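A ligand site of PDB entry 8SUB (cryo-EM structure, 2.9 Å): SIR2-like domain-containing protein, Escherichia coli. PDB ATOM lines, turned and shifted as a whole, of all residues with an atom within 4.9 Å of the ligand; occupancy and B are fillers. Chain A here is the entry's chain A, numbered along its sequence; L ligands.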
ATOM      1  N   GLY A  33     -11.182  21.806  -0.982  1.00  0.00           N
ATOM      2  CA  GLY A  33     -11.270  21.268  -2.327  1.00  0.00           C
ATOM      3  C   GLY A  33      -9.953  21.265  -3.074  1.00  0.00           C
ATOM      4  O   GLY A  33      -8.890  21.334  -2.467  1.00  0.00           O
ATOM      5  N   ALA A  34     -10.015  21.218  -4.410  1.00  0.00           N
ATOM      6  CA  ALA A  34      -8.811  21.053  -5.202  1.00  0.00           C
ATOM      7  C   ALA A  34      -7.973  22.314  -5.312  1.00  0.00           C
ATOM      8  O   ALA A  34      -6.785  22.224  -5.598  1.00  0.00           O
ATOM      9  CB  ALA A  34      -9.163  20.566  -6.611  1.00  0.00           C
ATOM     10  N   GLY A  35      -8.574  23.479  -5.108  1.00  0.00           N
ATOM     11  CA  GLY A  35      -7.849  24.731  -5.190  1.00  0.00           C
ATOM     12  C   GLY A  35      -7.099  25.131  -3.956  1.00  0.00           C
ATOM     13  O   GLY A  35      -6.439  26.168  -3.961  1.00  0.00           O
ATOM     14  N   VAL A  38      -3.120  24.479  -4.526  1.00  0.00           N
ATOM     15  CA  VAL A  38      -2.467  25.124  -5.654  1.00  0.00           C
ATOM     16  C   VAL A  38      -1.239  25.914  -5.195  1.00  0.00           C
ATOM     17  O   VAL A  38      -0.235  25.979  -5.913  1.00  0.00           O
ATOM     18  CB  VAL A  38      -3.472  26.030  -6.397  1.00  0.00           C
ATOM     19  CG1 VAL A  38      -2.767  26.908  -7.400  1.00  0.00           C
ATOM     20  CG2 VAL A  38      -4.519  25.189  -7.080  1.00  0.00           C
ATOM     21  N   THR A  44      -5.467  22.310 -10.652  1.00  0.00           N
ATOM     22  CA  THR A  44      -6.900  22.065 -10.660  1.00  0.00           C
ATOM     23  C   THR A  44      -7.257  21.074 -11.776  1.00  0.00           C
ATOM     24  O   THR A  44      -6.384  20.501 -12.429  1.00  0.00           O
ATOM     25  CB  THR A  44      -7.654  23.382 -10.812  1.00  0.00           C
ATOM     26  OG1 THR A  44      -7.229  24.038 -12.014  1.00  0.00           O
ATOM     27  CG2 THR A  44      -7.379  24.286  -9.643  1.00  0.00           C
ATOM     28  N   MET A  45      -8.555  20.872 -12.002  1.00  0.00           N
ATOM     29  CA  MET A  45      -8.993  19.862 -12.972  1.00  0.00           C
ATOM     30  C   MET A  45      -8.850  20.346 -14.412  1.00  0.00           C
ATOM     31  O   MET A  45      -8.565  19.545 -15.310  1.00  0.00           O
ATOM     32  CB  MET A  45     -10.444  19.466 -12.694  1.00  0.00           C
ATOM     33  CG  MET A  45     -10.640  18.663 -11.423  1.00  0.00           C
ATOM     34  SD  MET A  45      -9.897  17.010 -11.489  1.00  0.00           S
ATOM     35  CE  MET A  45      -8.512  17.206 -10.377  1.00  0.00           C
ATOM     36  N   ASN A  81     -15.562  15.982 -16.138  1.00  0.00           N
ATOM     37  CA  ASN A  81     -15.422  15.409 -14.800  1.00  0.00           C
ATOM     38  C   ASN A  81     -14.474  14.210 -14.904  1.00  0.00           C
ATOM     39  O   ASN A  81     -14.837  13.178 -15.462  1.00  0.00           O
ATOM     40  CB  ASN A  81     -16.781  14.998 -14.251  1.00  0.00           C
ATOM     41  CG  ASN A  81     -16.812  14.893 -12.749  1.00  0.00           C
ATOM     42  OD1 ASN A  81     -15.814  14.535 -12.122  1.00  0.00           O
ATOM     43  ND2 ASN A  81     -17.950  15.183 -12.154  1.00  0.00           N
ATOM     44  N   GLU A  83     -12.671  12.234 -12.528  1.00  0.00           N
ATOM     45  CA  GLU A  83     -12.799  11.044 -11.714  1.00  0.00           C
ATOM     46  C   GLU A  83     -14.096  10.290 -11.951  1.00  0.00           C
ATOM     47  O   GLU A  83     -14.248   9.175 -11.463  1.00  0.00           O
ATOM     48  CB  GLU A  83     -12.684  11.378 -10.228  1.00  0.00           C
ATOM     49  CG  GLU A  83     -13.774  12.260  -9.700  1.00  0.00           C
ATOM     50  CD  GLU A  83     -13.420  13.710  -9.797  1.00  0.00           C
ATOM     51  OE1 GLU A  83     -12.567  14.057 -10.622  1.00  0.00           O
ATOM     52  OE2 GLU A  83     -13.993  14.505  -9.037  1.00  0.00           O
ATOM     53  N   THR A 167     -11.517  16.569  -0.530  1.00  0.00           N
ATOM     54  CA  THR A 167     -11.594  15.804  -1.769  1.00  0.00           C
ATOM     55  C   THR A 167     -10.236  15.703  -2.468  1.00  0.00           C
ATOM     56  O   THR A 167     -10.180  15.328  -3.637  1.00  0.00           O
ATOM     57  CB  THR A 167     -12.614  16.410  -2.729  1.00  0.00           C
ATOM     58  OG1 THR A 167     -12.080  17.599  -3.311  1.00  0.00           O
ATOM     59  CG2 THR A 167     -13.892  16.753  -2.017  1.00  0.00           C
ATOM     60  N   HIS A 227     -12.333  10.837  -1.498  1.00  0.00           N
ATOM     61  CA  HIS A 227     -12.028  10.221  -2.779  1.00  0.00           C
ATOM     62  C   HIS A 227     -10.920   9.173  -2.682  1.00  0.00           C
ATOM     63  O   HIS A 227     -10.384   8.754  -3.705  1.00  0.00           O
ATOM     64  CB  HIS A 227     -11.637  11.268  -3.822  1.00  0.00           C
ATOM     65  CG  HIS A 227     -12.810  11.985  -4.420  1.00  0.00           C
ATOM     66  ND1 HIS A 227     -14.043  11.394  -4.588  1.00  0.00           N
ATOM     67  CD2 HIS A 227     -12.924  13.239  -4.915  1.00  0.00           C
ATOM     68  CE1 HIS A 227     -14.871  12.259  -5.143  1.00  0.00           C
ATOM     69  NE2 HIS A 227     -14.219  13.393  -5.344  1.00  0.00           N
ATOM     70  N   ASN A 305     -13.910  26.218   1.410  1.00  0.00           N
ATOM     71  CA  ASN A 305     -12.905  26.926   0.621  1.00  0.00           C
ATOM     72  C   ASN A 305     -12.296  25.968  -0.397  1.00  0.00           C
ATOM     73  O   ASN A 305     -11.987  24.821  -0.055  1.00  0.00           O
ATOM     74  CB  ASN A 305     -11.808  27.505   1.519  1.00  0.00           C
ATOM     75  CG  ASN A 305     -10.862  28.436   0.775  1.00  0.00           C
ATOM     76  OD1 ASN A 305      -9.938  27.975   0.106  1.00  0.00           O
ATOM     77  ND2 ASN A 305     -11.076  29.730   0.887  1.00  0.00           N
ATOM     78  N   GLY A 306     -12.114  26.429  -1.629  1.00  0.00           N
ATOM     79  CA  GLY A 306     -11.484  25.647  -2.669  1.00  0.00           C
ATOM     80  C   GLY A 306     -12.407  24.751  -3.476  1.00  0.00           C
ATOM     81  O   GLY A 306     -11.941  24.095  -4.405  1.00  0.00           O
ATOM     82  N   PHE A 307     -13.702  24.725  -3.161  1.00  0.00           N
ATOM     83  CA  PHE A 307     -14.648  23.806  -3.764  1.00  0.00           C
ATOM     84  C   PHE A 307     -15.336  24.472  -4.949  1.00  0.00           C
ATOM     85  O   PHE A 307     -15.695  25.646  -4.895  1.00  0.00           O
ATOM     86  CB  PHE A 307     -15.671  23.366  -2.715  1.00  0.00           C
ATOM     87  CG  PHE A 307     -16.566  22.249  -3.151  1.00  0.00           C
ATOM     88  CD1 PHE A 307     -16.050  21.090  -3.683  1.00  0.00           C
ATOM     89  CD2 PHE A 307     -17.936  22.340  -2.987  1.00  0.00           C
ATOM     90  CE1 PHE A 307     -16.876  20.066  -4.070  1.00  0.00           C
ATOM     91  CE2 PHE A 307     -18.770  21.320  -3.370  1.00  0.00           C
ATOM     92  CZ  PHE A 307     -18.234  20.186  -3.912  1.00  0.00           C
ATOM     93  N   GLY A 308     -15.522  23.714  -6.027  1.00  0.00           N
ATOM     94  CA  GLY A 308     -16.076  24.252  -7.251  1.00  0.00           C
ATOM     95  C   GLY A 308     -17.573  24.142  -7.408  1.00  0.00           C
ATOM     96  O   GLY A 308     -18.146  24.681  -8.358  1.00  0.00           O
ATOM     97  N   GLY A 310     -19.460  21.615  -8.182  1.00  0.00           N
ATOM     98  CA  GLY A 310     -19.872  20.792  -9.292  1.00  0.00           C
ATOM     99  C   GLY A 310     -20.329  19.395  -8.959  1.00  0.00           C
ATOM    100  O   GLY A 310     -20.424  18.554  -9.859  1.00  0.00           O
ATOM    101  N   ASP A 311     -20.630  19.112  -7.688  1.00  0.00           N
ATOM    102  CA  ASP A 311     -21.081  17.802  -7.247  1.00  0.00           C
ATOM    103  C   ASP A 311     -22.543  17.893  -6.844  1.00  0.00           C
ATOM    104  O   ASP A 311     -22.911  18.739  -6.030  1.00  0.00           O
ATOM    105  CB  ASP A 311     -20.231  17.300  -6.074  1.00  0.00           C
ATOM    106  CG  ASP A 311     -20.209  15.789  -5.978  1.00  0.00           C
ATOM    107  OD1 ASP A 311     -21.237  15.145  -6.280  1.00  0.00           O
ATOM    108  OD2 ASP A 311     -19.168  15.239  -5.587  1.00  0.00           O
ATOM    109  N   ILE A 314     -23.400  16.398  -2.869  1.00  0.00           N
ATOM    110  CA  ILE A 314     -22.986  17.319  -1.819  1.00  0.00           C
ATOM    111  C   ILE A 314     -23.858  18.556  -1.811  1.00  0.00           C
ATOM    112  O   ILE A 314     -24.221  19.070  -0.746  1.00  0.00           O
ATOM    113  CB  ILE A 314     -21.493  17.677  -1.980  1.00  0.00           C
ATOM    114  CG1 ILE A 314     -20.616  16.478  -1.647  1.00  0.00           C
ATOM    115  CG2 ILE A 314     -21.122  18.839  -1.099  1.00  0.00           C
ATOM    116  CD1 ILE A 314     -19.154  16.687  -1.957  1.00  0.00           C
ATOM    117  N   TYR A 333     -15.887  32.047  -2.878  1.00  0.00           N
ATOM    118  CA  TYR A 333     -16.022  31.823  -4.318  1.00  0.00           C
ATOM    119  C   TYR A 333     -15.290  32.942  -5.060  1.00  0.00           C
ATOM    120  O   TYR A 333     -15.802  34.060  -5.161  1.00  0.00           O
ATOM    121  CB  TYR A 333     -17.485  31.760  -4.739  1.00  0.00           C
ATOM    122  CG  TYR A 333     -17.705  31.062  -6.060  1.00  0.00           C
ATOM    123  CD1 TYR A 333     -17.636  29.688  -6.164  1.00  0.00           C
ATOM    124  CD2 TYR A 333     -17.990  31.786  -7.210  1.00  0.00           C
ATOM    125  CE1 TYR A 333     -17.839  29.046  -7.367  1.00  0.00           C
ATOM    126  CE2 TYR A 333     -18.195  31.158  -8.408  1.00  0.00           C
ATOM    127  CZ  TYR A 333     -18.121  29.800  -8.489  1.00  0.00           C
ATOM    128  OH  TYR A 333     -18.329  29.174  -9.696  1.00  0.00           O
ATOM    129  N   PRO A 334     -14.093  32.670  -5.590  1.00  0.00           N
ATOM    130  CA  PRO A 334     -13.273  33.764  -6.148  1.00  0.00           C
ATOM    131  C   PRO A 334     -13.903  34.520  -7.302  1.00  0.00           C
ATOM    132  O   PRO A 334     -13.683  35.735  -7.406  1.00  0.00           O
ATOM    133  CB  PRO A 334     -11.993  33.028  -6.571  1.00  0.00           C
ATOM    134  CG  PRO A 334     -11.925  31.848  -5.700  1.00  0.00           C
ATOM    135  CD  PRO A 334     -13.350  31.404  -5.528  1.00  0.00           C
ATOM    136  N   GLU A 335     -14.649  33.869  -8.187  1.00  0.00           N
ATOM    137  CA  GLU A 335     -15.161  34.520  -9.392  1.00  0.00           C
ATOM    138  C   GLU A 335     -16.690  34.542  -9.354  1.00  0.00           C
ATOM    139  O   GLU A 335     -17.354  33.734  -9.993  1.00  0.00           O
ATOM    140  CB  GLU A 335     -14.649  33.818 -10.646  1.00  0.00           C
ATOM    141  CG  GLU A 335     -14.628  32.308 -10.550  1.00  0.00           C
ATOM    142  CD  GLU A 335     -13.821  31.665 -11.654  1.00  0.00           C
ATOM    143  OE1 GLU A 335     -13.191  32.409 -12.438  1.00  0.00           O
ATOM    144  OE2 GLU A 335     -13.800  30.419 -11.742  1.00  0.00           O
ATOM    145  N   ALA A 375     -10.506  35.865  -1.903  1.00  0.00           N
ATOM    146  CA  ALA A 375     -11.146  34.611  -1.524  1.00  0.00           C
ATOM    147  C   ALA A 375     -10.212  33.420  -1.730  1.00  0.00           C
ATOM    148  O   ALA A 375     -10.655  32.325  -2.057  1.00  0.00           O
ATOM    149  CB  ALA A 375     -12.436  34.414  -2.318  1.00  0.00           C
ATOM    150  N   TYR A 376      -8.913  33.626  -1.535  1.00  0.00           N
ATOM    151  CA  TYR A 376      -7.919  32.579  -1.686  1.00  0.00           C
ATOM    152  C   TYR A 376      -7.630  31.933  -0.333  1.00  0.00           C
ATOM    153  O   TYR A 376      -8.068  32.410   0.710  1.00  0.00           O
ATOM    154  CB  TYR A 376      -6.652  33.155  -2.315  1.00  0.00           C
ATOM    155  CG  TYR A 376      -6.696  33.210  -3.821  1.00  0.00           C
ATOM    156  CD1 TYR A 376      -7.852  32.916  -4.518  1.00  0.00           C
ATOM    157  CD2 TYR A 376      -5.575  33.557  -4.548  1.00  0.00           C
ATOM    158  CE1 TYR A 376      -7.896  32.955  -5.889  1.00  0.00           C
ATOM    159  CE2 TYR A 376      -5.601  33.609  -5.920  1.00  0.00           C
ATOM    160  CZ  TYR A 376      -6.762  33.303  -6.587  1.00  0.00           C
ATOM    161  OH  TYR A 376      -6.806  33.342  -7.958  1.00  0.00           O
ATOM    162  N   PHE A 377      -6.905  30.804  -0.368  1.00  0.00           N
ATOM    163  CA  PHE A 377      -6.663  30.039   0.847  1.00  0.00           C
ATOM    164  C   PHE A 377      -5.839  30.827   1.866  1.00  0.00           C
ATOM    165  O   PHE A 377      -6.163  30.841   3.063  1.00  0.00           O
ATOM    166  CB  PHE A 377      -5.966  28.724   0.479  1.00  0.00           C
ATOM    167  CG  PHE A 377      -5.796  27.776   1.631  1.00  0.00           C
ATOM    168  CD1 PHE A 377      -6.884  27.111   2.166  1.00  0.00           C
ATOM    169  CD2 PHE A 377      -4.556  27.534   2.180  1.00  0.00           C
ATOM    170  CE1 PHE A 377      -6.727  26.241   3.214  1.00  0.00           C
ATOM    171  CE2 PHE A 377      -4.397  26.675   3.221  1.00  0.00           C
ATOM    172  CZ  PHE A 377      -5.483  26.021   3.747  1.00  0.00           C
HETATM  173  N1  LIG L   1      -7.317  29.382  -3.689  1.00  0.00           N
HETATM  174  C1  LIG L   1      -8.588  29.041  -3.563  1.00  0.00           C
HETATM  175  N2  LIG L   1      -9.429  28.692  -4.501  1.00  0.00           N
HETATM  176  C2  LIG L   1      -8.867  28.683  -5.708  1.00  0.00           C
HETATM  177  C3  LIG L   1      -7.562  29.012  -5.996  1.00  0.00           C
HETATM  178  C4  LIG L   1      -6.755  29.373  -4.896  1.00  0.00           C
HETATM  179  N3  LIG L   1      -5.479  29.712  -5.035  1.00  0.00           N
HETATM  180  N4  LIG L   1      -7.310  28.905  -7.338  1.00  0.00           N
HETATM  181  C5  LIG L   1      -8.440  28.526  -7.840  1.00  0.00           C
HETATM  182  N5  LIG L   1      -9.427  28.368  -6.906  1.00  0.00           N
HETATM  183  P1  LIG L   1     -12.144  22.340  -9.010  1.00  0.00           P
HETATM  184  P2  LIG L   1     -13.342  20.499  -7.084  1.00  0.00           P
HETATM  185  C6  LIG L   1     -10.796  27.952  -7.127  1.00  0.00           C
HETATM  186  O1  LIG L   1     -13.425  22.250  -9.767  1.00  0.00           O
HETATM  187  O2  LIG L   1     -14.482  20.491  -8.039  1.00  0.00           O
HETATM  188  C7  LIG L   1     -16.234  16.345  -8.339  1.00  0.00           C
HETATM  189  O3  LIG L   1     -17.313  17.177  -8.503  1.00  0.00           O
HETATM  190  C8  LIG L   1     -11.213  27.900  -8.593  1.00  0.00           C
HETATM  191  O4  LIG L   1     -11.545  29.176  -9.032  1.00  0.00           O
HETATM  192  O5  LIG L   1     -10.871  22.421  -9.765  1.00  0.00           O
HETATM  193  O6  LIG L   1     -13.537  21.019  -5.709  1.00  0.00           O
HETATM  194  C9  LIG L   1     -16.071  15.929  -6.879  1.00  0.00           C
HETATM  195  O7  LIG L   1     -16.972  16.575  -6.037  1.00  0.00           O
HETATM  196  C10 LIG L   1     -12.387  26.924  -8.517  1.00  0.00           C
HETATM  197  O8  LIG L   1     -13.530  27.562  -8.019  1.00  0.00           O
HETATM  198  O9  LIG L   1     -12.066  21.210  -7.829  1.00  0.00           O
HETATM  199  C11 LIG L   1     -14.676  16.440  -6.509  1.00  0.00           C
HETATM  200  O10 LIG L   1     -14.587  16.949  -5.215  1.00  0.00           O
HETATM  201  C12 LIG L   1     -11.905  25.930  -7.484  1.00  0.00           C
HETATM  202  O11 LIG L   1     -10.930  26.629  -6.712  1.00  0.00           O
HETATM  203  C13 LIG L   1     -14.460  17.548  -7.531  1.00  0.00           C
HETATM  204  O12 LIG L   1     -15.032  16.994  -8.694  1.00  0.00           O
HETATM  205  C14 LIG L   1     -11.335  24.672  -8.112  1.00  0.00           C
HETATM  206  O13 LIG L   1     -12.236  23.602  -7.954  1.00  0.00           O
HETATM  207  C15 LIG L   1     -13.018  17.931  -7.757  1.00  0.00           C
HETATM  208  O14 LIG L   1     -12.627  19.021  -6.944  1.00  0.00           O
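The side-chain carboxylate (OE2) of Glu 83 lies close to an oxygen (O12) of the ligand, 2.7 Å away. An oxygen (O6) of the ligand lies within hydrogen-bond range of the backbone NH of Gly 308, 3.4 Å away. The side-chain carboxylate of Asp 311 lies within hydrogen-bond range of an oxygen (O7) of the ligand, at 2.6 Å. An oxygen (O10) of the ligand is in hydrogen-bond range of the side-chain hydroxyl (OG1) of Thr 167.
The backbone carbonyl oxygen (O) of Gly 306 sits at hydrogen-bond distance from the backbone NH (N) of Ala 34 (3.5 Å). The backbone carbonyl oxygen (O) of Gly 306 sits at hydrogen-bond distance from the backbone NH (N) of Gly 35 (3.5 Å).
N1 of the ligand lies close to O of Gly 35 (3.3 Å). Residues that only touch the ligand: Ala 34 (3.2 Å), Phe 307 (3.2 Å), His 227 (3.3 Å), Thr 44 (3.5 Å), Gly 306 (3.6 Å), Met 45 (3.6 Å), Phe 377 (3.6 Å), Gly 310 (3.7 Å), Tyr 376 (3.7 Å) and Glu 335 (3.7 Å). 15 residues have an atom within 4 Å of the ligand: Ala 34, Gly 35, Thr 44, Met 45, Glu 83, Thr 167, His 227, Gly 306, Phe 307, Gly 308, Gly 310, Asp 311, Glu 335, Tyr 376 and Phe 377. Along chain A the residues within 4 Å of the ligand span positions 34 to 377.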
